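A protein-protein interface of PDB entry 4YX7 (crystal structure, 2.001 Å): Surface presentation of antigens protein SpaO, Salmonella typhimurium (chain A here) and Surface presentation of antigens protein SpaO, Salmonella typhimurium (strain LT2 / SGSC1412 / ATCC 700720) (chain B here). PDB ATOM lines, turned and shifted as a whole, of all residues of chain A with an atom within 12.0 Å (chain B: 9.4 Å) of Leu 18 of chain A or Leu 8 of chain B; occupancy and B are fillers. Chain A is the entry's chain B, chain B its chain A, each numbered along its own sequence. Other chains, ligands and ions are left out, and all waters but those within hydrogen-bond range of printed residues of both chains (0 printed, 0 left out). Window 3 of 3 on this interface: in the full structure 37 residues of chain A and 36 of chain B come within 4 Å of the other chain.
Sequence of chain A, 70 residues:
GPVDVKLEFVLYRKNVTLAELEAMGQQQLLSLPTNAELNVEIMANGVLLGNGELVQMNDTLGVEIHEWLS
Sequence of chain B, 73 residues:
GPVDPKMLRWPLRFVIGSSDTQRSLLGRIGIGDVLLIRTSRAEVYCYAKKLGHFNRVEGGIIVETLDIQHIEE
N of Trp 10 of chain B is in hydrogen-bond range of O of Val 16 of chain A (2.5 Å). N of Leu 12 of chain B is in hydrogen-bond range of O of Lys 14 of chain A (2.9 Å).
O of Trp 10 of chain B touches O of Lys 14 of chain A, 3.6 Å away. Pro 11 of chain B touches Lys 14 of chain A. Asn 15 of chain A touches Trp 10 of chain B. O of Val 16 of chain A touches CA of Arg 9 of chain B, 3.1 Å away. Leu 18 of chain A touches Leu 8 of chain B (N to O, 3.9 Å). Leu 21 of chain A touches Leu 12 of chain B. O of Leu 21 of chain A touches CD1 of Leu 66 of chain B, at 3.0 Å. SD of Met 24 of chain A touches CD1 of Leu 12 of chain B, 3.8 Å away. CD1 of Leu 66 of chain B touches CG of Met 24 of chain A, at 3.6 Å. Leu 66 of chain B touches Gly 25 of chain A (CD1 to N, 3.4 Å).
The side-chain amino group of Lys 14 of chain A lies within salt-bridge range of the side-chain carboxylate of Glu 20 of chain A (3.99 Å). OG1 of Thr 17 of chain A sits close to N of Ala 19 of chain A (3.4 Å). OG1 of Thr 17 of chain A sits at hydrogen-bond distance from N of Glu 20 of chain A (3.1 Å). The backbone carbonyl oxygen (O) of Gly 25 of chain A lies within hydrogen-bond range of the side-chain amide nitrogen (NE2) of Gln 27 of chain A (3.5 Å).
Of the 12 printed residues of chain B, 6 touch a printed residue of chain A. Hydrophobic or aromatic side chains of chain B within 4 Å of the printed part of chain A: Trp 10, Leu 12 and Leu 66. Among the printed residues, no Asp or Glu carboxylate lies within 4 Å of a Lys or Arg side-chain nitrogen of the other chain.
Printed residues of chain B within 4 Å of Val 16 of chain A: Arg 9 (3.1 Å) and Trp 10 (2.5 Å). Leu 18 of chain A touches just one residue of chain B: Leu 8. Glu 20 of chain A touches none of the printed residues of chain B. No residue of chain A comes within 4 Å of Met 7 of chain B. Of chain A, only Thr 17 and Leu 18 come within 4 Å of Leu 8 of chain B. Of the printed residues of chain A, Pro 11 of chain B touches Lys 14 (3.8 Å). Of the printed residues of chain A, Leu 12 of chain B touches Lys 14 (2.9 Å), Leu 21 (3.8 Å) and Met 24 (3.8 Å). The nearest residue of chain A that does not touch Leu 8 of chain B is Val 16 of chain A (4.1 Å). The nearest printed residue of chain B that does not touch Leu 21 of chain A is Trp 10 of chain B (4.1 Å).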
ATOM      1  N   LYS A  14      -0.628  10.536  31.041  1.00  0.00           N
ATOM      2  CA  LYS A  14      -0.171  11.444  29.986  1.00  0.00           C
ATOM      3  C   LYS A  14      -1.258  11.568  28.917  1.00  0.00           C
ATOM      4  O   LYS A  14      -1.812  10.562  28.480  1.00  0.00           O
ATOM      5  CB  LYS A  14       1.143  10.934  29.369  1.00  0.00           C
ATOM      6  CG  LYS A  14       1.903  11.929  28.476  1.00  0.00           C
ATOM      7  CD  LYS A  14       2.184  13.258  29.189  1.00  0.00           C
ATOM      8  CE  LYS A  14       3.009  14.240  28.349  1.00  0.00           C
ATOM      9  NZ  LYS A  14       3.862  13.601  27.302  1.00  0.00           N
ATOM     10  N   ASN A  15      -1.578  12.799  28.521  1.00  0.00           N
ATOM     11  CA  ASN A  15      -2.471  13.046  27.385  1.00  0.00           C
ATOM     12  C   ASN A  15      -1.691  13.063  26.070  1.00  0.00           C
ATOM     13  O   ASN A  15      -0.803  13.894  25.864  1.00  0.00           O
ATOM     14  CB  ASN A  15      -3.237  14.362  27.556  1.00  0.00           C
ATOM     15  CG  ASN A  15      -4.586  14.178  28.222  1.00  0.00           C
ATOM     16  OD1 ASN A  15      -4.723  14.357  29.432  1.00  0.00           O
ATOM     17  ND2 ASN A  15      -5.596  13.838  27.429  1.00  0.00           N
ATOM     18  N   VAL A  16      -2.046  12.153  25.174  1.00  0.00           N
ATOM     19  CA  VAL A  16      -1.205  11.850  24.034  1.00  0.00           C
ATOM     20  C   VAL A  16      -1.943  12.047  22.713  1.00  0.00           C
ATOM     21  O   VAL A  16      -3.146  11.812  22.622  1.00  0.00           O
ATOM     22  CB  VAL A  16      -0.654  10.396  24.170  1.00  0.00           C
ATOM     23  CG1 VAL A  16      -1.040   9.517  22.990  1.00  0.00           C
ATOM     24  CG2 VAL A  16       0.850  10.411  24.380  1.00  0.00           C
ATOM     25  N   THR A  17      -1.216  12.512  21.700  1.00  0.00           N
ATOM     26  CA  THR A  17      -1.752  12.660  20.356  1.00  0.00           C
ATOM     27  C   THR A  17      -1.521  11.357  19.616  1.00  0.00           C
ATOM     28  O   THR A  17      -0.803  10.498  20.107  1.00  0.00           O
ATOM     29  CB  THR A  17      -1.081  13.811  19.593  1.00  0.00           C
ATOM     30  OG1 THR A  17       0.296  13.494  19.376  1.00  0.00           O
ATOM     31  CG2 THR A  17      -1.159  15.096  20.386  1.00  0.00           C
ATOM     32  N   LEU A  18      -2.105  11.204  18.434  1.00  0.00           N
ATOM     33  CA  LEU A  18      -1.879   9.984  17.670  1.00  0.00           C
ATOM     34  C   LEU A  18      -0.393   9.853  17.333  1.00  0.00           C
ATOM     35  O   LEU A  18       0.169   8.753  17.365  1.00  0.00           O
ATOM     36  CB  LEU A  18      -2.728   9.971  16.400  1.00  0.00           C
ATOM     37  CG  LEU A  18      -2.770   8.649  15.624  1.00  0.00           C
ATOM     38  CD1 LEU A  18      -4.145   8.459  15.017  1.00  0.00           C
ATOM     39  CD2 LEU A  18      -1.706   8.584  14.529  1.00  0.00           C
ATOM     40  N   ALA A  19       0.232  10.989  17.026  1.00  0.00           N
ATOM     41  CA  ALA A  19       1.658  11.049  16.717  1.00  0.00           C
ATOM     42  C   ALA A  19       2.493  10.544  17.873  1.00  0.00           C
ATOM     43  O   ALA A  19       3.291   9.628  17.706  1.00  0.00           O
ATOM     44  CB  ALA A  19       2.065  12.464  16.368  1.00  0.00           C
ATOM     45  N   GLU A  20       2.314  11.156  19.041  1.00  0.00           N
ATOM     46  CA  GLU A  20       2.985  10.708  20.261  1.00  0.00           C
ATOM     47  C   GLU A  20       2.686   9.235  20.520  1.00  0.00           C
ATOM     48  O   GLU A  20       3.534   8.500  21.021  1.00  0.00           O
ATOM     49  CB  GLU A  20       2.555  11.544  21.475  1.00  0.00           C
ATOM     50  CG  GLU A  20       3.034  12.998  21.488  1.00  0.00           C
ATOM     51  CD  GLU A  20       2.799  13.692  22.838  1.00  0.00           C
ATOM     52  OE1 GLU A  20       1.668  13.628  23.362  1.00  0.00           O
ATOM     53  OE2 GLU A  20       3.748  14.303  23.380  1.00  0.00           O
ATOM     54  N   LEU A  21       1.479   8.814  20.146  1.00  0.00           N
ATOM     55  CA  LEU A  21       1.009   7.447  20.381  1.00  0.00           C
ATOM     56  C   LEU A  21       1.738   6.433  19.505  1.00  0.00           C
ATOM     57  O   LEU A  21       2.138   5.381  19.982  1.00  0.00           O
ATOM     58  CB  LEU A  21      -0.504   7.368  20.150  1.00  0.00           C
ATOM     59  CG  LEU A  21      -1.306   6.215  20.746  1.00  0.00           C
ATOM     60  CD1 LEU A  21      -0.951   5.979  22.202  1.00  0.00           C
ATOM     61  CD2 LEU A  21      -2.787   6.509  20.602  1.00  0.00           C
ATOM     62  N   GLU A  22       1.926   6.752  18.230  1.00  0.00           N
ATOM     63  CA  GLU A  22       2.663   5.863  17.339  1.00  0.00           C
ATOM     64  C   GLU A  22       4.178   5.918  17.596  1.00  0.00           C
ATOM     65  O   GLU A  22       4.889   4.939  17.374  1.00  0.00           O
ATOM     66  CB  GLU A  22       2.357   6.205  15.878  1.00  0.00           C
ATOM     67  CG  GLU A  22       2.953   7.515  15.407  1.00  0.00           C
ATOM     68  CD  GLU A  22       2.439   7.940  14.052  1.00  0.00           C
ATOM     69  OE1 GLU A  22       1.503   7.301  13.532  1.00  0.00           O
ATOM     70  OE2 GLU A  22       2.984   8.911  13.499  1.00  0.00           O
ATOM     71  N   ALA A  23       4.663   7.067  18.066  1.00  0.00           N
ATOM     72  CA  ALA A  23       6.067   7.227  18.434  1.00  0.00           C
ATOM     73  C   ALA A  23       6.366   6.391  19.666  1.00  0.00           C
ATOM     74  O   ALA A  23       7.436   5.797  19.801  1.00  0.00           O
ATOM     75  CB  ALA A  23       6.392   8.686  18.694  1.00  0.00           C
ATOM     76  N   MET A  24       5.397   6.361  20.568  1.00  0.00           N
ATOM     77  CA  MET A  24       5.434   5.491  21.733  1.00  0.00           C
ATOM     78  C   MET A  24       5.263   4.030  21.328  1.00  0.00           C
ATOM     79  O   MET A  24       5.852   3.133  21.935  1.00  0.00           O
ATOM     80  CB  MET A  24       4.337   5.907  22.703  1.00  0.00           C
ATOM     81  CG  MET A  24       4.213   5.083  23.948  1.00  0.00           C
ATOM     82  SD  MET A  24       2.907   5.829  24.930  1.00  0.00           S
ATOM     83  CE  MET A  24       3.459   7.531  24.918  1.00  0.00           C
ATOM     84  N   GLY A  25       4.459   3.809  20.290  1.00  0.00           N
ATOM     85  CA  GLY A  25       4.182   2.478  19.784  1.00  0.00           C
ATOM     86  C   GLY A  25       5.450   1.798  19.329  1.00  0.00           C
ATOM     87  O   GLY A  25       5.540   0.572  19.311  1.00  0.00           O
ATOM     88  N   GLN A  26       6.440   2.608  18.967  1.00  0.00           N
ATOM     89  CA  GLN A  26       7.753   2.082  18.628  1.00  0.00           C
ATOM     90  C   GLN A  26       8.828   2.521  19.636  1.00  0.00           C
ATOM     91  O   GLN A  26       9.761   3.247  19.305  1.00  0.00           O
ATOM     92  CB  GLN A  26       8.122   2.467  17.187  1.00  0.00           C
ATOM     93  CG  GLN A  26       8.067   3.942  16.843  1.00  0.00           C
ATOM     94  CD  GLN A  26       8.188   4.156  15.355  1.00  0.00           C
ATOM     95  OE1 GLN A  26       8.209   3.194  14.585  1.00  0.00           O
ATOM     96  NE2 GLN A  26       8.301   5.413  14.938  1.00  0.00           N
ATOM     97  N   GLN A  27       8.653   2.049  20.872  1.00  0.00           N
ATOM     98  CA  GLN A  27       9.645   2.099  21.960  1.00  0.00           C
ATOM     99  C   GLN A  27      10.467   3.378  22.077  1.00  0.00           C
ATOM    100  O   GLN A  27      11.691   3.328  22.175  1.00  0.00           O
ATOM    101  CB  GLN A  27      10.612   0.908  21.856  1.00  0.00           C
ATOM    102  CG  GLN A  27       9.984  -0.399  21.365  1.00  0.00           C
ATOM    103  CD  GLN A  27       9.737  -0.448  19.862  1.00  0.00           C
ATOM    104  OE1 GLN A  27      10.527   0.073  19.068  1.00  0.00           O
ATOM    105  NE2 GLN A  27       8.626  -1.066  19.467  1.00  0.00           N
ATOM    106  N   GLN A  28       9.790   4.519  22.078  1.00  0.00           N
ATOM    107  CA  GLN A  28      10.439   5.779  22.391  1.00  0.00           C
ATOM    108  C   GLN A  28      10.283   6.080  23.873  1.00  0.00           C
ATOM    109  O   GLN A  28       9.167   6.100  24.399  1.00  0.00           O
ATOM    110  CB  GLN A  28       9.858   6.910  21.557  1.00  0.00           C
ATOM    111  CG  GLN A  28      10.265   8.282  22.030  1.00  0.00           C
ATOM    112  CD  GLN A  28       9.779   9.365  21.103  1.00  0.00           C
ATOM    113  OE1 GLN A  28       9.502  10.483  21.531  1.00  0.00           O
ATOM    114  NE2 GLN A  28       9.671   9.041  19.818  1.00  0.00           N
ATOM    115  N   LEU A  30       9.650   7.218  27.362  1.00  0.00           N
ATOM    116  CA  LEU A  30       8.824   8.178  28.073  1.00  0.00           C
ATOM    117  C   LEU A  30       9.468   8.484  29.429  1.00  0.00           C
ATOM    118  O   LEU A  30       9.550   7.625  30.300  1.00  0.00           O
ATOM    119  CB  LEU A  30       7.407   7.639  28.227  1.00  0.00           C
ATOM    120  CG  LEU A  30       6.343   8.686  28.509  1.00  0.00           C
ATOM    121  CD1 LEU A  30       5.024   8.198  27.979  1.00  0.00           C
ATOM    122  CD2 LEU A  30       6.244   8.931  29.996  1.00  0.00           C
ATOM    123  N   PRO B   5     -16.010  15.582  16.051  1.00  0.00           N
ATOM    124  CA  PRO B   5     -15.844  14.470  15.107  1.00  0.00           C
ATOM    125  C   PRO B   5     -14.821  13.450  15.608  1.00  0.00           C
ATOM    126  O   PRO B   5     -15.100  12.734  16.566  1.00  0.00           O
ATOM    127  CB  PRO B   5     -15.359  15.164  13.830  1.00  0.00           C
ATOM    128  N   LYS B   6     -13.655  13.389  14.972  1.00  0.00           N
ATOM    129  CA  LYS B   6     -12.595  12.486  15.405  1.00  0.00           C
ATOM    130  C   LYS B   6     -12.064  12.929  16.762  1.00  0.00           C
ATOM    131  O   LYS B   6     -12.252  14.074  17.158  1.00  0.00           O
ATOM    132  CB  LYS B   6     -11.465  12.452  14.373  1.00  0.00           C
ATOM    133  N   MET B   7     -11.408  12.024  17.482  1.00  0.00           N
ATOM    134  CA  MET B   7     -10.742  12.407  18.726  1.00  0.00           C
ATOM    135  C   MET B   7      -9.239  12.651  18.510  1.00  0.00           C
ATOM    136  O   MET B   7      -8.544  11.892  17.829  1.00  0.00           O
ATOM    137  CB  MET B   7     -10.989  11.361  19.821  1.00  0.00           C
ATOM    138  CG  MET B   7     -10.788   9.910  19.411  1.00  0.00           C
ATOM    139  SD  MET B   7     -11.138   8.745  20.761  1.00  0.00           S
ATOM    140  CE  MET B   7     -10.697   9.704  22.207  1.00  0.00           C
ATOM    141  N   LEU B   8      -8.765  13.750  19.088  1.00  0.00           N
ATOM    142  CA  LEU B   8      -7.416  14.261  18.851  1.00  0.00           C
ATOM    143  C   LEU B   8      -6.371  13.700  19.819  1.00  0.00           C
ATOM    144  O   LEU B   8      -5.318  13.219  19.398  1.00  0.00           O
ATOM    145  CB  LEU B   8      -7.424  15.793  18.943  1.00  0.00           C
ATOM    146  CG  LEU B   8      -8.147  16.607  17.872  1.00  0.00           C
ATOM    147  CD1 LEU B   8      -8.410  18.004  18.400  1.00  0.00           C
ATOM    148  CD2 LEU B   8      -7.313  16.666  16.598  1.00  0.00           C
ATOM    149  N   ARG B   9      -6.669  13.780  21.114  1.00  0.00           N
ATOM    150  CA  ARG B   9      -5.757  13.324  22.159  1.00  0.00           C
ATOM    151  C   ARG B   9      -6.348  12.197  23.033  1.00  0.00           C
ATOM    152  O   ARG B   9      -7.563  12.120  23.264  1.00  0.00           O
ATOM    153  CB  ARG B   9      -5.340  14.507  23.034  1.00  0.00           C
ATOM    154  N   TRP B  10      -5.467  11.332  23.528  1.00  0.00           N
ATOM    155  CA  TRP B  10      -5.881  10.114  24.204  1.00  0.00           C
ATOM    156  C   TRP B  10      -5.254  10.033  25.584  1.00  0.00           C
ATOM    157  O   TRP B  10      -4.037  10.066  25.711  1.00  0.00           O
ATOM    158  CB  TRP B  10      -5.486   8.882  23.380  1.00  0.00           C
ATOM    159  CG  TRP B  10      -5.813   8.972  21.907  1.00  0.00           C
ATOM    160  CD1 TRP B  10      -5.232   9.793  20.982  1.00  0.00           C
ATOM    161  CD2 TRP B  10      -6.768   8.185  21.192  1.00  0.00           C
ATOM    162  NE1 TRP B  10      -5.781   9.584  19.748  1.00  0.00           N
ATOM    163  CE2 TRP B  10      -6.727   8.596  19.846  1.00  0.00           C
ATOM    164  CE3 TRP B  10      -7.665   7.174  21.561  1.00  0.00           C
ATOM    165  CZ2 TRP B  10      -7.543   8.037  18.865  1.00  0.00           C
ATOM    166  CZ3 TRP B  10      -8.478   6.616  20.585  1.00  0.00           C
ATOM    167  CH2 TRP B  10      -8.410   7.051  19.252  1.00  0.00           C
ATOM    168  N   PRO B  11      -6.085   9.901  26.626  1.00  0.00           N
ATOM    169  CA  PRO B  11      -5.582   9.875  27.999  1.00  0.00           C
ATOM    170  C   PRO B  11      -5.029   8.513  28.384  1.00  0.00           C
ATOM    171  O   PRO B  11      -5.818   7.596  28.596  1.00  0.00           O
ATOM    172  CB  PRO B  11      -6.830  10.202  28.823  1.00  0.00           C
ATOM    173  CG  PRO B  11      -7.932   9.636  28.031  1.00  0.00           C
ATOM    174  CD  PRO B  11      -7.548   9.754  26.580  1.00  0.00           C
ATOM    175  N   LEU B  12      -3.712   8.371  28.493  1.00  0.00           N
ATOM    176  CA  LEU B  12      -3.160   7.067  28.843  1.00  0.00           C
ATOM    177  C   LEU B  12      -2.867   6.951  30.337  1.00  0.00           C
ATOM    178  O   LEU B  12      -2.458   7.911  30.978  1.00  0.00           O
ATOM    179  CB  LEU B  12      -1.895   6.784  28.042  1.00  0.00           C
ATOM    180  CG  LEU B  12      -1.985   6.918  26.524  1.00  0.00           C
ATOM    181  CD1 LEU B  12      -0.671   6.537  25.909  1.00  0.00           C
ATOM    182  CD2 LEU B  12      -3.096   6.065  25.964  1.00  0.00           C
ATOM    183  N   TYR B  47      -8.786   4.651  28.880  1.00  0.00           N
ATOM    184  CA  TYR B  47     -10.082   4.274  29.430  1.00  0.00           C
ATOM    185  C   TYR B  47     -10.073   2.776  29.782  1.00  0.00           C
ATOM    186  O   TYR B  47      -9.144   2.299  30.422  1.00  0.00           O
ATOM    187  CB  TYR B  47     -11.203   4.643  28.444  1.00  0.00           C
ATOM    188  CG  TYR B  47     -11.197   6.120  28.075  1.00  0.00           C
ATOM    189  CD1 TYR B  47     -11.609   7.080  28.987  1.00  0.00           C
ATOM    190  CD2 TYR B  47     -10.774   6.553  26.826  1.00  0.00           C
ATOM    191  CE1 TYR B  47     -11.607   8.423  28.669  1.00  0.00           C
ATOM    192  CE2 TYR B  47     -10.768   7.896  26.502  1.00  0.00           C
ATOM    193  CZ  TYR B  47     -11.190   8.822  27.433  1.00  0.00           C
ATOM    194  OH  TYR B  47     -11.194  10.162  27.136  1.00  0.00           O
ATOM    195  N   LEU B  66       1.155  -1.246  22.220  1.00  0.00           N
ATOM    196  CA  LEU B  66       0.207  -0.263  21.695  1.00  0.00           C
ATOM    197  C   LEU B  66      -0.527  -0.821  20.485  1.00  0.00           C
ATOM    198  O   LEU B  66      -0.203  -0.505  19.340  1.00  0.00           O
ATOM    199  CB  LEU B  66       0.895   1.061  21.350  1.00  0.00           C
ATOM    200  CG  LEU B  66       1.181   1.937  22.571  1.00  0.00           C
ATOM    201  CD1 LEU B  66       1.615   3.315  22.163  1.00  0.00           C
ATOM    202  CD2 LEU B  66      -0.036   2.029  23.462  1.00  0.00           C
ATOM    203  N   ILE B  68      -3.955  -0.379  18.854  1.00  0.00           N
ATOM    204  CA  ILE B  68      -4.937   0.709  18.940  1.00  0.00           C
ATOM    205  C   ILE B  68      -6.240   0.539  18.115  1.00  0.00           C
ATOM    206  O   ILE B  68      -7.075   1.452  18.068  1.00  0.00           O
ATOM    207  CB  ILE B  68      -4.282   2.043  18.525  1.00  0.00           C
ATOM    208  N   GLN B  69      -6.425  -0.615  17.479  1.00  0.00           N
ATOM    209  CA  GLN B  69      -7.641  -0.867  16.713  1.00  0.00           C
ATOM    210  C   GLN B  69      -7.867  -2.357  16.501  1.00  0.00           C
ATOM    211  O   GLN B  69      -6.933  -3.101  16.204  1.00  0.00           O
ATOM    212  CB  GLN B  69      -7.580  -0.151  15.362  1.00  0.00           C
